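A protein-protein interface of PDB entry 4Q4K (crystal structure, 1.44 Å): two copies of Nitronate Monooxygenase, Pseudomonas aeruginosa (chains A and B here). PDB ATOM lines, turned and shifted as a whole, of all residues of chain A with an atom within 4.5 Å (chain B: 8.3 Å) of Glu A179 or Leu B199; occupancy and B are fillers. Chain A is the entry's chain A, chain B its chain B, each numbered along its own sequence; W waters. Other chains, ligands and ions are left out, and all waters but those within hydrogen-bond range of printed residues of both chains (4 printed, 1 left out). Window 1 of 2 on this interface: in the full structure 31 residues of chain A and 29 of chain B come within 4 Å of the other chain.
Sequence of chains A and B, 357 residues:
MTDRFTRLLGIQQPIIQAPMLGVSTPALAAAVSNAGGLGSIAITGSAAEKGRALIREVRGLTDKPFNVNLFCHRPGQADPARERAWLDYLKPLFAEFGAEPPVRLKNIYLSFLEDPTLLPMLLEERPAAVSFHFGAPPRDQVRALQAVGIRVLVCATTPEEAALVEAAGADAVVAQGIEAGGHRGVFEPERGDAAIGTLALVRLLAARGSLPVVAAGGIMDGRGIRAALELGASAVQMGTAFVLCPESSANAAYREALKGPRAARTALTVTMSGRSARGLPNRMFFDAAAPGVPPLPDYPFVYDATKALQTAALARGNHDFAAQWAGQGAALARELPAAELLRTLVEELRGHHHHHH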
ATOM      1  N   GLY A 177      30.239 -28.960  -6.209  1.00  0.00           N
ATOM      2  CA  GLY A 177      29.253 -28.074  -6.767  1.00  0.00           C
ATOM      3  C   GLY A 177      29.665 -26.653  -6.469  1.00  0.00           C
ATOM      4  O   GLY A 177      30.539 -26.353  -5.640  1.00  0.00           O
ATOM      5  N   ILE A 178      28.934 -25.693  -7.074  1.00  0.00           N
ATOM      6  CA  ILE A 178      29.160 -24.226  -6.909  1.00  0.00           C
ATOM      7  C   ILE A 178      28.997 -23.801  -5.447  1.00  0.00           C
ATOM      8  O   ILE A 178      29.687 -22.846  -5.055  1.00  0.00           O
ATOM      9  CB  ILE A 178      28.268 -23.418  -7.895  1.00  0.00           C
ATOM     10  CG1 ILE A 178      28.867 -22.024  -8.177  1.00  0.00           C
ATOM     11  CG2 ILE A 178      26.822 -23.298  -7.435  1.00  0.00           C
ATOM     12  CD1 ILE A 178      30.319 -21.895  -8.577  1.00  0.00           C
ATOM     13  N   GLU A 179      28.158 -24.534  -4.738  1.00  0.00           N
ATOM     14  CA  GLU A 179      27.920 -24.206  -3.307  1.00  0.00           C
ATOM     15  C   GLU A 179      29.169 -24.303  -2.483  1.00  0.00           C
ATOM     16  O   GLU A 179      29.189 -23.754  -1.401  1.00  0.00           O
ATOM     17  CB  GLU A 179      26.911 -25.199  -2.757  1.00  0.00           C
ATOM     18  CG  GLU A 179      25.505 -24.995  -3.231  1.00  0.00           C
ATOM     19  CD  GLU A 179      25.107 -25.775  -4.453  1.00  0.00           C
ATOM     20  OE1 GLU A 179      25.932 -26.036  -5.348  1.00  0.00           O
ATOM     21  OE2 GLU A 179      23.899 -26.036  -4.458  1.00  0.00           O
ATOM     22  N   ALA A 180      30.207 -25.044  -2.898  1.00  0.00           N
ATOM     23  CA  ALA A 180      31.295 -25.354  -1.982  1.00  0.00           C
ATOM     24  C   ALA A 180      32.091 -24.179  -1.540  1.00  0.00           C
ATOM     25  O   ALA A 180      32.288 -23.189  -2.286  1.00  0.00           O
ATOM     26  CB  ALA A 180      32.246 -26.320  -2.696  1.00  0.00           C
ATOM     27  N   GLY A 181      32.541 -24.295  -0.275  1.00  0.00           N
ATOM     28  CA  GLY A 181      33.468 -23.363   0.274  1.00  0.00           C
ATOM     29  C   GLY A 181      34.890 -23.549  -0.213  1.00  0.00           C
ATOM     30  O   GLY A 181      35.256 -24.652  -0.644  1.00  0.00           O
ATOM     31  N   GLY A 197      25.958 -26.333 -10.195  1.00  0.00           N
ATOM     32  CA  GLY A 197      25.462 -26.558  -8.812  1.00  0.00           C
ATOM     33  C   GLY A 197      25.567 -28.005  -8.404  1.00  0.00           C
ATOM     34  O   GLY A 197      25.520 -28.930  -9.223  1.00  0.00           O
ATOM     35  N   THR A 198      25.658 -28.229  -7.121  1.00  0.00           N
ATOM     36  CA  THR A 198      25.706 -29.579  -6.584  1.00  0.00           C
ATOM     37  C   THR A 198      24.624 -30.498  -7.013  1.00  0.00           C
ATOM     38  O   THR A 198      24.912 -31.656  -7.394  1.00  0.00           O
ATOM     39  CB  THR A 198      25.698 -29.510  -5.051  1.00  0.00           C
ATOM     40  OG1 THR A 198      26.853 -28.771  -4.648  1.00  0.00           O
ATOM     41  CG2 THR A 198      25.810 -30.938  -4.425  1.00  0.00           C
ATOM     42  N   LEU A 199      23.380 -30.071  -7.047  1.00  0.00           N
ATOM     43  CA  LEU A 199      22.228 -30.944  -7.353  1.00  0.00           C
ATOM     44  C   LEU A 199      22.394 -31.454  -8.808  1.00  0.00           C
ATOM     45  O   LEU A 199      22.193 -32.657  -9.075  1.00  0.00           O
ATOM     46  CB  LEU A 199      20.912 -30.217  -7.090  1.00  0.00           C
ATOM     47  CG  LEU A 199      19.662 -31.031  -7.477  1.00  0.00           C
ATOM     48  CD1 LEU A 199      18.647 -30.791  -6.404  1.00  0.00           C
ATOM     49  CD2 LEU A 199      19.124 -30.552  -8.824  1.00  0.00           C
ATOM     50  N   GLY A 217      29.565 -29.719  -1.423  1.00  0.00           N
ATOM     51  CA  GLY A 217      29.152 -28.337  -1.651  1.00  0.00           C
ATOM     52  C   GLY A 217      27.747 -28.087  -1.142  1.00  0.00           C
ATOM     53  O   GLY A 217      26.762 -28.509  -1.737  1.00  0.00           O
ATOM     54  N   GLY A 218      27.671 -27.335  -0.027  1.00  0.00           N
ATOM     55  CA  GLY A 218      26.402 -26.868   0.531  1.00  0.00           C
ATOM     56  C   GLY A 218      25.719 -27.798   1.510  1.00  0.00           C
ATOM     57  O   GLY A 218      24.623 -27.425   1.984  1.00  0.00           O
ATOM     58  N   ILE A 219      26.307 -28.944   1.787  1.00  0.00           N
ATOM     59  CA  ILE A 219      25.660 -29.987   2.611  1.00  0.00           C
ATOM     60  C   ILE A 219      26.032 -29.696   4.087  1.00  0.00           C
ATOM     61  O   ILE A 219      27.192 -29.683   4.446  1.00  0.00           O
ATOM     62  CB  ILE A 219      26.098 -31.402   2.205  1.00  0.00           C
ATOM     63  CG1 ILE A 219      25.607 -31.679   0.752  1.00  0.00           C
ATOM     64  CG2 ILE A 219      25.526 -32.482   3.121  1.00  0.00           C
ATOM     65  CD1 ILE A 219      26.390 -32.745   0.049  1.00  0.00           C
ATOM     66  N   ARG A 278      35.634 -19.537  -2.651  1.00  0.00           N
ATOM     67  CA  ARG A 278      34.385 -18.992  -2.072  1.00  0.00           C
ATOM     68  C   ARG A 278      34.574 -18.755  -0.571  1.00  0.00           C
ATOM     69  O   ARG A 278      34.964 -19.605   0.163  1.00  0.00           O
ATOM     70  CB  ARG A 278      33.260 -20.005  -2.222  1.00  0.00           C
ATOM     71  CG  ARG A 278      31.935 -19.434  -1.638  1.00  0.00           C
ATOM     72  CD  ARG A 278      30.766 -20.417  -1.732  1.00  0.00           C
ATOM     73  NE  ARG A 278      30.448 -20.617  -3.183  1.00  0.00           N
ATOM     74  CZ  ARG A 278      29.944 -19.690  -3.979  1.00  0.00           C
ATOM     75  NH1 ARG A 278      29.556 -18.472  -3.534  1.00  0.00           N
ATOM     76  NH2 ARG A 278      29.752 -19.978  -5.300  1.00  0.00           N
ATOM     77  N   GLY A 327      31.057 -22.283   2.482  1.00  0.00           N
ATOM     78  CA  GLY A 327      30.087 -22.685   1.473  1.00  0.00           C
ATOM     79  C   GLY A 327      28.774 -21.929   1.512  1.00  0.00           C
ATOM     80  O   GLY A 327      28.459 -21.166   2.455  1.00  0.00           O
ATOM     81  N   GLN A 328      27.930 -22.150   0.527  1.00  0.00           N
ATOM     82  CA  GLN A 328      26.660 -21.434   0.472  1.00  0.00           C
ATOM     83  C   GLN A 328      25.632 -21.891   1.547  1.00  0.00           C
ATOM     84  O   GLN A 328      24.613 -21.187   1.671  1.00  0.00           O
ATOM     85  CB  GLN A 328      26.033 -21.542  -0.945  1.00  0.00           C
ATOM     86  CG  GLN A 328      26.851 -20.702  -1.914  1.00  0.00           C
ATOM     87  CD  GLN A 328      26.319 -20.763  -3.376  1.00  0.00           C
ATOM     88  OE1 GLN A 328      25.674 -21.748  -3.751  1.00  0.00           O
ATOM     89  NE2 GLN A 328      26.559 -19.744  -4.160  1.00  0.00           N
ATOM     90  N   ALA B 175      11.944 -21.400  -5.175  1.00  0.00           N
ATOM     91  CA  ALA B 175      13.394 -21.225  -4.892  1.00  0.00           C
ATOM     92  C   ALA B 175      14.170 -21.599  -6.187  1.00  0.00           C
ATOM     93  O   ALA B 175      14.276 -22.808  -6.482  1.00  0.00           O
ATOM     94  CB  ALA B 175      13.854 -22.119  -3.796  1.00  0.00           C
ATOM     95  N   GLN B 176      14.639 -20.638  -6.964  1.00  0.00           N
ATOM     96  CA  GLN B 176      15.346 -20.892  -8.243  1.00  0.00           C
ATOM     97  C   GLN B 176      16.831 -20.890  -8.012  1.00  0.00           C
ATOM     98  O   GLN B 176      17.414 -19.868  -7.710  1.00  0.00           O
ATOM     99  CB  GLN B 176      14.914 -19.867  -9.260  1.00  0.00           C
ATOM    100  CG  GLN B 176      15.492 -20.187 -10.652  1.00  0.00           C
ATOM    101  CD  GLN B 176      15.540 -18.997 -11.608  1.00  0.00           C
ATOM    102  OE1 GLN B 176      16.061 -17.925 -11.222  1.00  0.00           O
ATOM    103  NE2 GLN B 176      15.075 -19.141 -12.844  1.00  0.00           N
ATOM    104  N   GLY B 177      17.442 -22.100  -8.042  1.00  0.00           N
ATOM    105  CA  GLY B 177      18.881 -22.329  -7.975  1.00  0.00           C
ATOM    106  C   GLY B 177      19.607 -21.927  -9.265  1.00  0.00           C
ATOM    107  O   GLY B 177      19.048 -21.728 -10.348  1.00  0.00           O
ATOM    108  N   ILE B 178      20.899 -21.858  -9.067  1.00  0.00           N
ATOM    109  CA  ILE B 178      21.778 -21.529 -10.217  1.00  0.00           C
ATOM    110  C   ILE B 178      21.670 -22.510 -11.426  1.00  0.00           C
ATOM    111  O   ILE B 178      21.801 -22.091 -12.596  1.00  0.00           O
ATOM    112  CB  ILE B 178      23.227 -21.392  -9.758  1.00  0.00           C
ATOM    113  CG1 ILE B 178      24.050 -20.554 -10.803  1.00  0.00           C
ATOM    114  CG2 ILE B 178      23.862 -22.766  -9.593  1.00  0.00           C
ATOM    115  CD1 ILE B 178      23.571 -19.151 -11.060  1.00  0.00           C
ATOM    116  N   GLU B 179      21.275 -23.721 -11.104  1.00  0.00           N
ATOM    117  CA  GLU B 179      21.053 -24.704 -12.203  1.00  0.00           C
ATOM    118  C   GLU B 179      19.987 -24.416 -13.143  1.00  0.00           C
ATOM    119  O   GLU B 179      19.884 -25.010 -14.220  1.00  0.00           O
ATOM    120  CB  GLU B 179      20.691 -26.021 -11.534  1.00  0.00           C
ATOM    121  CG  GLU B 179      21.823 -26.702 -10.756  1.00  0.00           C
ATOM    122  CD  GLU B 179      21.883 -26.392  -9.307  1.00  0.00           C
ATOM    123  OE1 GLU B 179      21.423 -25.298  -8.871  1.00  0.00           O
ATOM    124  OE2 GLU B 179      22.336 -27.308  -8.599  1.00  0.00           O
ATOM    125  N   ALA B 194      24.065 -13.324  -6.099  1.00  0.00           N
ATOM    126  CA  ALA B 194      24.694 -14.313  -5.222  1.00  0.00           C
ATOM    127  C   ALA B 194      24.913 -15.728  -5.878  1.00  0.00           C
ATOM    128  O   ALA B 194      25.711 -16.535  -5.385  1.00  0.00           O
ATOM    129  CB  ALA B 194      23.878 -14.443  -3.947  1.00  0.00           C
ATOM    130  N   ALA B 195      24.109 -16.010  -6.918  1.00  0.00           N
ATOM    131  CA  ALA B 195      24.260 -17.239  -7.730  1.00  0.00           C
ATOM    132  C   ALA B 195      24.334 -18.461  -6.827  1.00  0.00           C
ATOM    133  O   ALA B 195      25.293 -19.231  -6.845  1.00  0.00           O
ATOM    134  CB  ALA B 195      25.487 -17.160  -8.705  1.00  0.00           C
ATOM    135  N   ILE B 196      23.279 -18.681  -6.007  1.00  0.00           N
ATOM    136  CA  ILE B 196      23.177 -19.812  -5.084  1.00  0.00           C
ATOM    137  C   ILE B 196      22.594 -21.096  -5.727  1.00  0.00           C
ATOM    138  O   ILE B 196      21.639 -21.013  -6.478  1.00  0.00           O
ATOM    139  CB  ILE B 196      22.317 -19.445  -3.758  1.00  0.00           C
ATOM    140  CG1 ILE B 196      22.840 -18.125  -3.133  1.00  0.00           C
ATOM    141  CG2 ILE B 196      22.266 -20.569  -2.726  1.00  0.00           C
ATOM    142  CD1 ILE B 196      21.895 -17.485  -2.113  1.00  0.00           C
ATOM    143  N   GLY B 197      23.295 -22.191  -5.482  1.00  0.00           N
ATOM    144  CA  GLY B 197      22.873 -23.503  -6.039  1.00  0.00           C
ATOM    145  C   GLY B 197      21.549 -23.986  -5.466  1.00  0.00           C
ATOM    146  O   GLY B 197      21.234 -23.629  -4.278  1.00  0.00           O
ATOM    147  N   THR B 198      20.782 -24.798  -6.186  1.00  0.00           N
ATOM    148  CA  THR B 198      19.478 -25.278  -5.729  1.00  0.00           C
ATOM    149  C   THR B 198      19.673 -25.965  -4.407  1.00  0.00           C
ATOM    150  O   THR B 198      18.830 -25.787  -3.514  1.00  0.00           O
ATOM    151  CB  THR B 198      18.915 -26.270  -6.756  1.00  0.00           C
ATOM    152  OG1 THR B 198      18.772 -25.548  -7.969  1.00  0.00           O
ATOM    153  CG2 THR B 198      17.529 -26.698  -6.370  1.00  0.00           C
ATOM    154  N   LEU B 199      20.695 -26.789  -4.188  1.00  0.00           N
ATOM    155  CA  LEU B 199      20.795 -27.607  -2.976  1.00  0.00           C
ATOM    156  C   LEU B 199      20.867 -26.675  -1.747  1.00  0.00           C
ATOM    157  O   LEU B 199      20.187 -26.956  -0.719  1.00  0.00           O
ATOM    158  CB  LEU B 199      21.957 -28.615  -3.062  1.00  0.00           C
ATOM    159  CG  LEU B 199      22.054 -29.537  -1.858  1.00  0.00           C
ATOM    160  CD1 LEU B 199      22.266 -30.973  -2.246  1.00  0.00           C
ATOM    161  CD2 LEU B 199      23.256 -29.050  -1.043  1.00  0.00           C
ATOM    162  N   ALA B 200      21.721 -25.675  -1.793  1.00  0.00           N
ATOM    163  CA  ALA B 200      21.808 -24.739  -0.687  1.00  0.00           C
ATOM    164  C   ALA B 200      20.541 -23.920  -0.616  1.00  0.00           C
ATOM    165  O   ALA B 200      20.001 -23.783   0.549  1.00  0.00           O
ATOM    166  CB  ALA B 200      23.035 -23.854  -0.811  1.00  0.00           C
ATOM    167  N   LEU B 201      20.001 -23.384  -1.700  1.00  0.00           N
ATOM    168  CA  LEU B 201      18.888 -22.392  -1.614  1.00  0.00           C
ATOM    169  C   LEU B 201      17.693 -23.083  -1.038  1.00  0.00           C
ATOM    170  O   LEU B 201      17.038 -22.509  -0.092  1.00  0.00           O
ATOM    171  CB  LEU B 201      18.590 -21.777  -2.964  1.00  0.00           C
ATOM    172  CG  LEU B 201      17.491 -20.723  -2.997  1.00  0.00           C
ATOM    173  CD1 LEU B 201      17.977 -19.537  -2.177  1.00  0.00           C
ATOM    174  CD2 LEU B 201      17.144 -20.328  -4.404  1.00  0.00           C
ATOM    175  N   VAL B 202      17.343 -24.268  -1.500  1.00  0.00           N
ATOM    176  CA  VAL B 202      16.089 -24.922  -1.053  1.00  0.00           C
ATOM    177  C   VAL B 202      16.207 -25.203   0.440  1.00  0.00           C
ATOM    178  O   VAL B 202      15.250 -24.928   1.170  1.00  0.00           O
ATOM    179  CB  VAL B 202      15.756 -26.186  -1.868  1.00  0.00           C
ATOM    180  CG1 VAL B 202      14.527 -26.885  -1.259  1.00  0.00           C
ATOM    181  CG2 VAL B 202      15.508 -25.766  -3.316  1.00  0.00           C
ATOM    182  N   ARG B 203      17.329 -25.723   0.921  1.00  0.00           N
ATOM    183  CA  ARG B 203      17.525 -26.032   2.355  1.00  0.00           C
ATOM    184  C   ARG B 203      17.449 -24.754   3.128  1.00  0.00           C
ATOM    185  O   ARG B 203      16.746 -24.711   4.183  1.00  0.00           O
ATOM    186  CB  ARG B 203      18.842 -26.787   2.571  1.00  0.00           C
ATOM    187  CG  ARG B 203      19.015 -27.306   4.001  1.00  0.00           C
ATOM    188  CD  ARG B 203      18.257 -28.621   4.162  1.00  0.00           C
ATOM    189  NE  ARG B 203      17.991 -28.869   5.580  1.00  0.00           N
ATOM    190  CZ  ARG B 203      16.860 -28.555   6.195  1.00  0.00           C
ATOM    191  NH1 ARG B 203      16.786 -28.805   7.506  1.00  0.00           N
ATOM    192  NH2 ARG B 203      15.816 -28.021   5.541  1.00  0.00           N
ATOM    193  N   LEU B 204      18.088 -23.688   2.665  1.00  0.00           N
ATOM    194  CA  LEU B 204      18.073 -22.429   3.407  1.00  0.00           C
ATOM    195  C   LEU B 204      16.630 -21.960   3.577  1.00  0.00           C
ATOM    196  O   LEU B 204      16.239 -21.630   4.716  1.00  0.00           O
ATOM    197  CB  LEU B 204      18.912 -21.370   2.735  1.00  0.00           C
ATOM    198  CG  LEU B 204      20.420 -21.657   2.868  1.00  0.00           C
ATOM    199  CD1 LEU B 204      21.158 -20.843   1.850  1.00  0.00           C
ATOM    200  CD2 LEU B 204      20.985 -21.243   4.245  1.00  0.00           C
ATOM    201  N   LEU B 205      15.876 -21.867   2.479  1.00  0.00           N
ATOM    202  CA  LEU B 205      14.476 -21.381   2.502  1.00  0.00           C
ATOM    203  C   LEU B 205      13.549 -22.326   3.258  1.00  0.00           C
ATOM    204  O   LEU B 205      12.651 -21.817   3.993  1.00  0.00           O
ATOM    205  CB  LEU B 205      13.939 -21.038   1.097  1.00  0.00           C
ATOM    206  CG  LEU B 205      14.632 -20.001   0.243  1.00  0.00           C
ATOM    207  CD1 LEU B 205      13.762 -19.556  -0.920  1.00  0.00           C
ATOM    208  CD2 LEU B 205      15.210 -18.832   1.020  1.00  0.00           C
ATOM    209  N   ALA B 206      13.733 -23.635   3.191  1.00  0.00           N
ATOM    210  CA  ALA B 206      12.903 -24.570   3.972  1.00  0.00           C
ATOM    211  C   ALA B 206      13.241 -24.488   5.456  1.00  0.00           C
ATOM    212  O   ALA B 206      12.324 -24.493   6.290  1.00  0.00           O
ATOM    213  CB  ALA B 206      12.996 -26.015   3.485  1.00  0.00           C
ATOM    214  N   ALA B 215      10.990 -26.087  -5.255  1.00  0.00           N
ATOM    215  CA  ALA B 215      12.397 -26.148  -5.733  1.00  0.00           C
ATOM    216  C   ALA B 215      12.429 -26.043  -7.252  1.00  0.00           C
ATOM    217  O   ALA B 215      11.737 -26.768  -7.929  1.00  0.00           O
ATOM    218  CB  ALA B 215      12.990 -27.454  -5.309  1.00  0.00           C
ATOM    219  N   ALA B 216      13.299 -25.177  -7.771  1.00  0.00           N
ATOM    220  CA  ALA B 216      13.387 -25.045  -9.255  1.00  0.00           C
ATOM    221  C   ALA B 216      14.854 -24.935  -9.598  1.00  0.00           C
ATOM    222  O   ALA B 216      15.569 -24.037  -9.157  1.00  0.00           O
ATOM    223  CB  ALA B 216      12.684 -23.777  -9.743  1.00  0.00           C
ATOM    224  N   GLY B 217      15.304 -25.830 -10.451  1.00  0.00           N
ATOM    225  CA  GLY B 217      16.630 -25.712 -11.123  1.00  0.00           C
ATOM    226  C   GLY B 217      17.371 -27.009 -11.031  1.00  0.00           C
ATOM    227  O   GLY B 217      17.806 -27.482  -9.995  1.00  0.00           O
ATOM    228  N   ALA B 227      15.148 -35.715  -3.983  1.00  0.00           N
ATOM    229  CA  ALA B 227      16.180 -34.984  -3.306  1.00  0.00           C
ATOM    230  C   ALA B 227      15.652 -33.651  -2.806  1.00  0.00           C
ATOM    231  O   ALA B 227      15.980 -33.196  -1.713  1.00  0.00           O
ATOM    232  CB  ALA B 227      17.360 -34.744  -4.250  1.00  0.00           C
ATOM    233  N   ALA B 228      14.902 -32.969  -3.659  1.00  0.00           N
ATOM    234  CA  ALA B 228      14.351 -31.667  -3.311  1.00  0.00           C
ATOM    235  C   ALA B 228      13.409 -31.785  -2.131  1.00  0.00           C
ATOM    236  O   ALA B 228      13.418 -30.897  -1.244  1.00  0.00           O
ATOM    237  CB  ALA B 228      13.622 -31.089  -4.523  1.00  0.00           C
ATOM    238  N   LEU B 231      15.239 -32.018   1.087  1.00  0.00           N
ATOM    239  CA  LEU B 231      15.839 -30.776   1.519  1.00  0.00           C
ATOM    240  C   LEU B 231      14.763 -29.899   2.156  1.00  0.00           C
ATOM    241  O   LEU B 231      15.045 -28.812   2.642  1.00  0.00           O
ATOM    242  CB  LEU B 231      16.441 -30.001   0.309  1.00  0.00           C
ATOM    243  CG  LEU B 231      17.681 -30.621  -0.326  1.00  0.00           C
ATOM    244  CD1 LEU B 231      17.972 -29.887  -1.649  1.00  0.00           C
ATOM    245  CD2 LEU B 231      18.853 -30.571   0.612  1.00  0.00           C
ATOM    246  N   GLY B 232      13.510 -30.350   2.081  1.00  0.00           N
ATOM    247  CA  GLY B 232      12.378 -29.656   2.742  1.00  0.00           C
ATOM    248  C   GLY B 232      11.464 -28.924   1.784  1.00  0.00           C
ATOM    249  O   GLY B 232      10.601 -28.121   2.171  1.00  0.00           O
ATOM    250  N   GLN B 328      21.053 -26.782 -16.048  1.00  0.00           N
ATOM    251  CA  GLN B 328      22.284 -27.565 -15.943  1.00  0.00           C
ATOM    252  C   GLN B 328      22.048 -29.074 -15.945  1.00  0.00           C
ATOM    253  O   GLN B 328      23.037 -29.782 -16.050  1.00  0.00           O
ATOM    254  CB  GLN B 328      23.038 -27.097 -14.702  1.00  0.00           C
ATOM    255  CG  GLN B 328      23.665 -25.732 -14.926  1.00  0.00           C
ATOM    256  CD  GLN B 328      24.498 -25.266 -13.733  1.00  0.00           C
ATOM    257  OE1 GLN B 328      24.287 -25.691 -12.570  1.00  0.00           O
ATOM    258  NE2 GLN B 328      25.465 -24.375 -14.006  1.00  0.00           N
HETATM  259  O   HOH W   1      26.644 -16.913  -2.896  1.00  0.00           O
HETATM  260  O   HOH W   2      21.934 -27.985   1.978  1.00  0.00           O
HETATM  261  O   HOH W   3      28.680 -16.680  -5.546  1.00  0.00           O
HETATM  262  O   HOH W   4      28.080 -18.699  -7.297  1.00  0.00           O
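N of Leu B199 lies within hydrogen-bond range of OE2 of Glu A179 (3.3 Å). OE2 of Glu A179 is in hydrogen-bond range of N of Ala B200. The backbone NH (N) of Gly A197 lies within hydrogen-bond range of the side-chain amide oxygen (OE1) of Gln B328. The backbone NH of Leu A199 lies within hydrogen-bond range of the side-chain carboxylate of Glu B179, at 3.3 Å. The side-chain amide nitrogen (NE2) of Gln A328 is in hydrogen-bond range of the backbone carbonyl oxygen (O) of Ala B195, 3.0 Å away. N of Gly B197 sits at hydrogen-bond distance from OE1 of Gln A328 (3.0 Å).
The backbone carbonyl oxygen of Ile A178 is in hydrogen-bond range of the guanidinium group of Arg A278 (2.9 Å). The side-chain carboxylate of Glu A179 lies within hydrogen-bond range of the backbone NH of Thr A198 (2.8 Å). O of Glu A179 is in hydrogen-bond range of N of Gln A328 (2.8 Å). The side-chain hydroxyl (OG1) of Thr A198 sits at hydrogen-bond distance from the backbone carbonyl oxygen (O) of Gly A217. The backbone carbonyl oxygen (O) of Glu B179 is in hydrogen-bond range of the backbone NH (N) of Gln B328 (2.8 Å). The side-chain hydroxyl (OG1) of Thr B198 lies within hydrogen-bond range of the backbone carbonyl oxygen (O) of Gly B217, 3.0 Å away.
Ile B178 touches Ile A178. Gly B197 touches Glu A179 (CA to OE2, 3.2 Å). N of Thr B198 touches OE2 of Glu A179, 3.8 Å away. Glu B179 touches Thr A198 (OE2 to N, 3.8 Å). Leu A199 touches Gly B217. Leu B199 touches Gly A218. CG1 of Ile A219 touches CD2 of Leu B199 (3.96 Å). Gln A328 touches Ala B194 (NE2 to O, 3.5 Å). Ile B196 touches Gln A328. Gln A328 touches Ala B200.
Glu A179 touches just these residues of chain B: Gly B197, Thr B198, Leu B199 and Ala B200. Ala A180 touches none of the printed residues of chain B. Gly A218 touches just one residue of chain B: Leu B199 (3.7 Å). Of the printed residues of chain A, Ile B196 touches Gln A328 (3.4 Å). Of chain A, only Glu A179 (3.3 Å), Gly A217 (3.6 Å), Gly A218 (3.7 Å) and Ile A219 (3.96 Å) come within 4 Å of Leu B199. Val B202 touches none of the printed residues of chain A. Of the printed residues of chain A, Leu B204 touches Gln A328 (3.5 Å). The nearest residue of chain B that does not touch Glu A179 is Glu B179 (4.6 Å). The nearest residue of chain A that does not touch Leu B199 is Thr A198 (4.2 Å).
Printed residues of chain A that touch a printed residue of chain B: Ile A178, Glu A179, Gly A197, Thr A198, Leu A199, Gly A217, Gly A218, Ile A219 and Gln A328. Printed residues of chain B that touch a printed residue of chain A: Ile B178, Glu B179, Ala B194, Ala B195, Ile B196, Gly B197, Thr B198, Leu B199, Ala B200, Leu B204, Gly B217 and Gln B328. Hydrophobic or aromatic side chains of chain B within 4 Å of the printed part of chain A: Ile B178, Ile B196, Leu B199, Ala B200 and Leu B204. Among the printed residues, 19 pairs touch across the chains.
Glu A179 touches Thr B198, and with the chains exchanged Thr A198 touches Glu B179. Glu A179 touches Leu B199, and with the chains exchanged Leu A199 touches Glu B179. Gly A197 touches Gln B328, and with the chains exchanged Gln A328 touches Gly B197. Leu A199 touches Gly B217, and with the chains exchanged Gly A217 touches Leu B199. Positions printed for both chains: 177, 178, 179, 197, 198, 199, 217 and 328. Of the 19 pairs that touch across the chains among the printed residues, 11 have their exchanged pair printed and touching as well.
Water W1 lies within hydrogen-bond range of the backbone carbonyl oxygen of Ala B194 (2.7 Å), the side-chain amide nitrogen of Gln A328 (3.1 Å) and the guanidinium group of Arg A278 (3.4 Å). Water W2 bridges the backbone carbonyl oxygen (O) of Gly A218 (2.7 Å) and the backbone carbonyl oxygen (O) of Leu B199 (3.4 Å). Water W3 lies within hydrogen-bond range of NH1 of Arg A278 (2.8 Å) and O of Ala B194 (3.0 Å). Water W4 bridges O of Ala B195 (2.9 Å) and NH2 of Arg A278 (2.9 Å).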
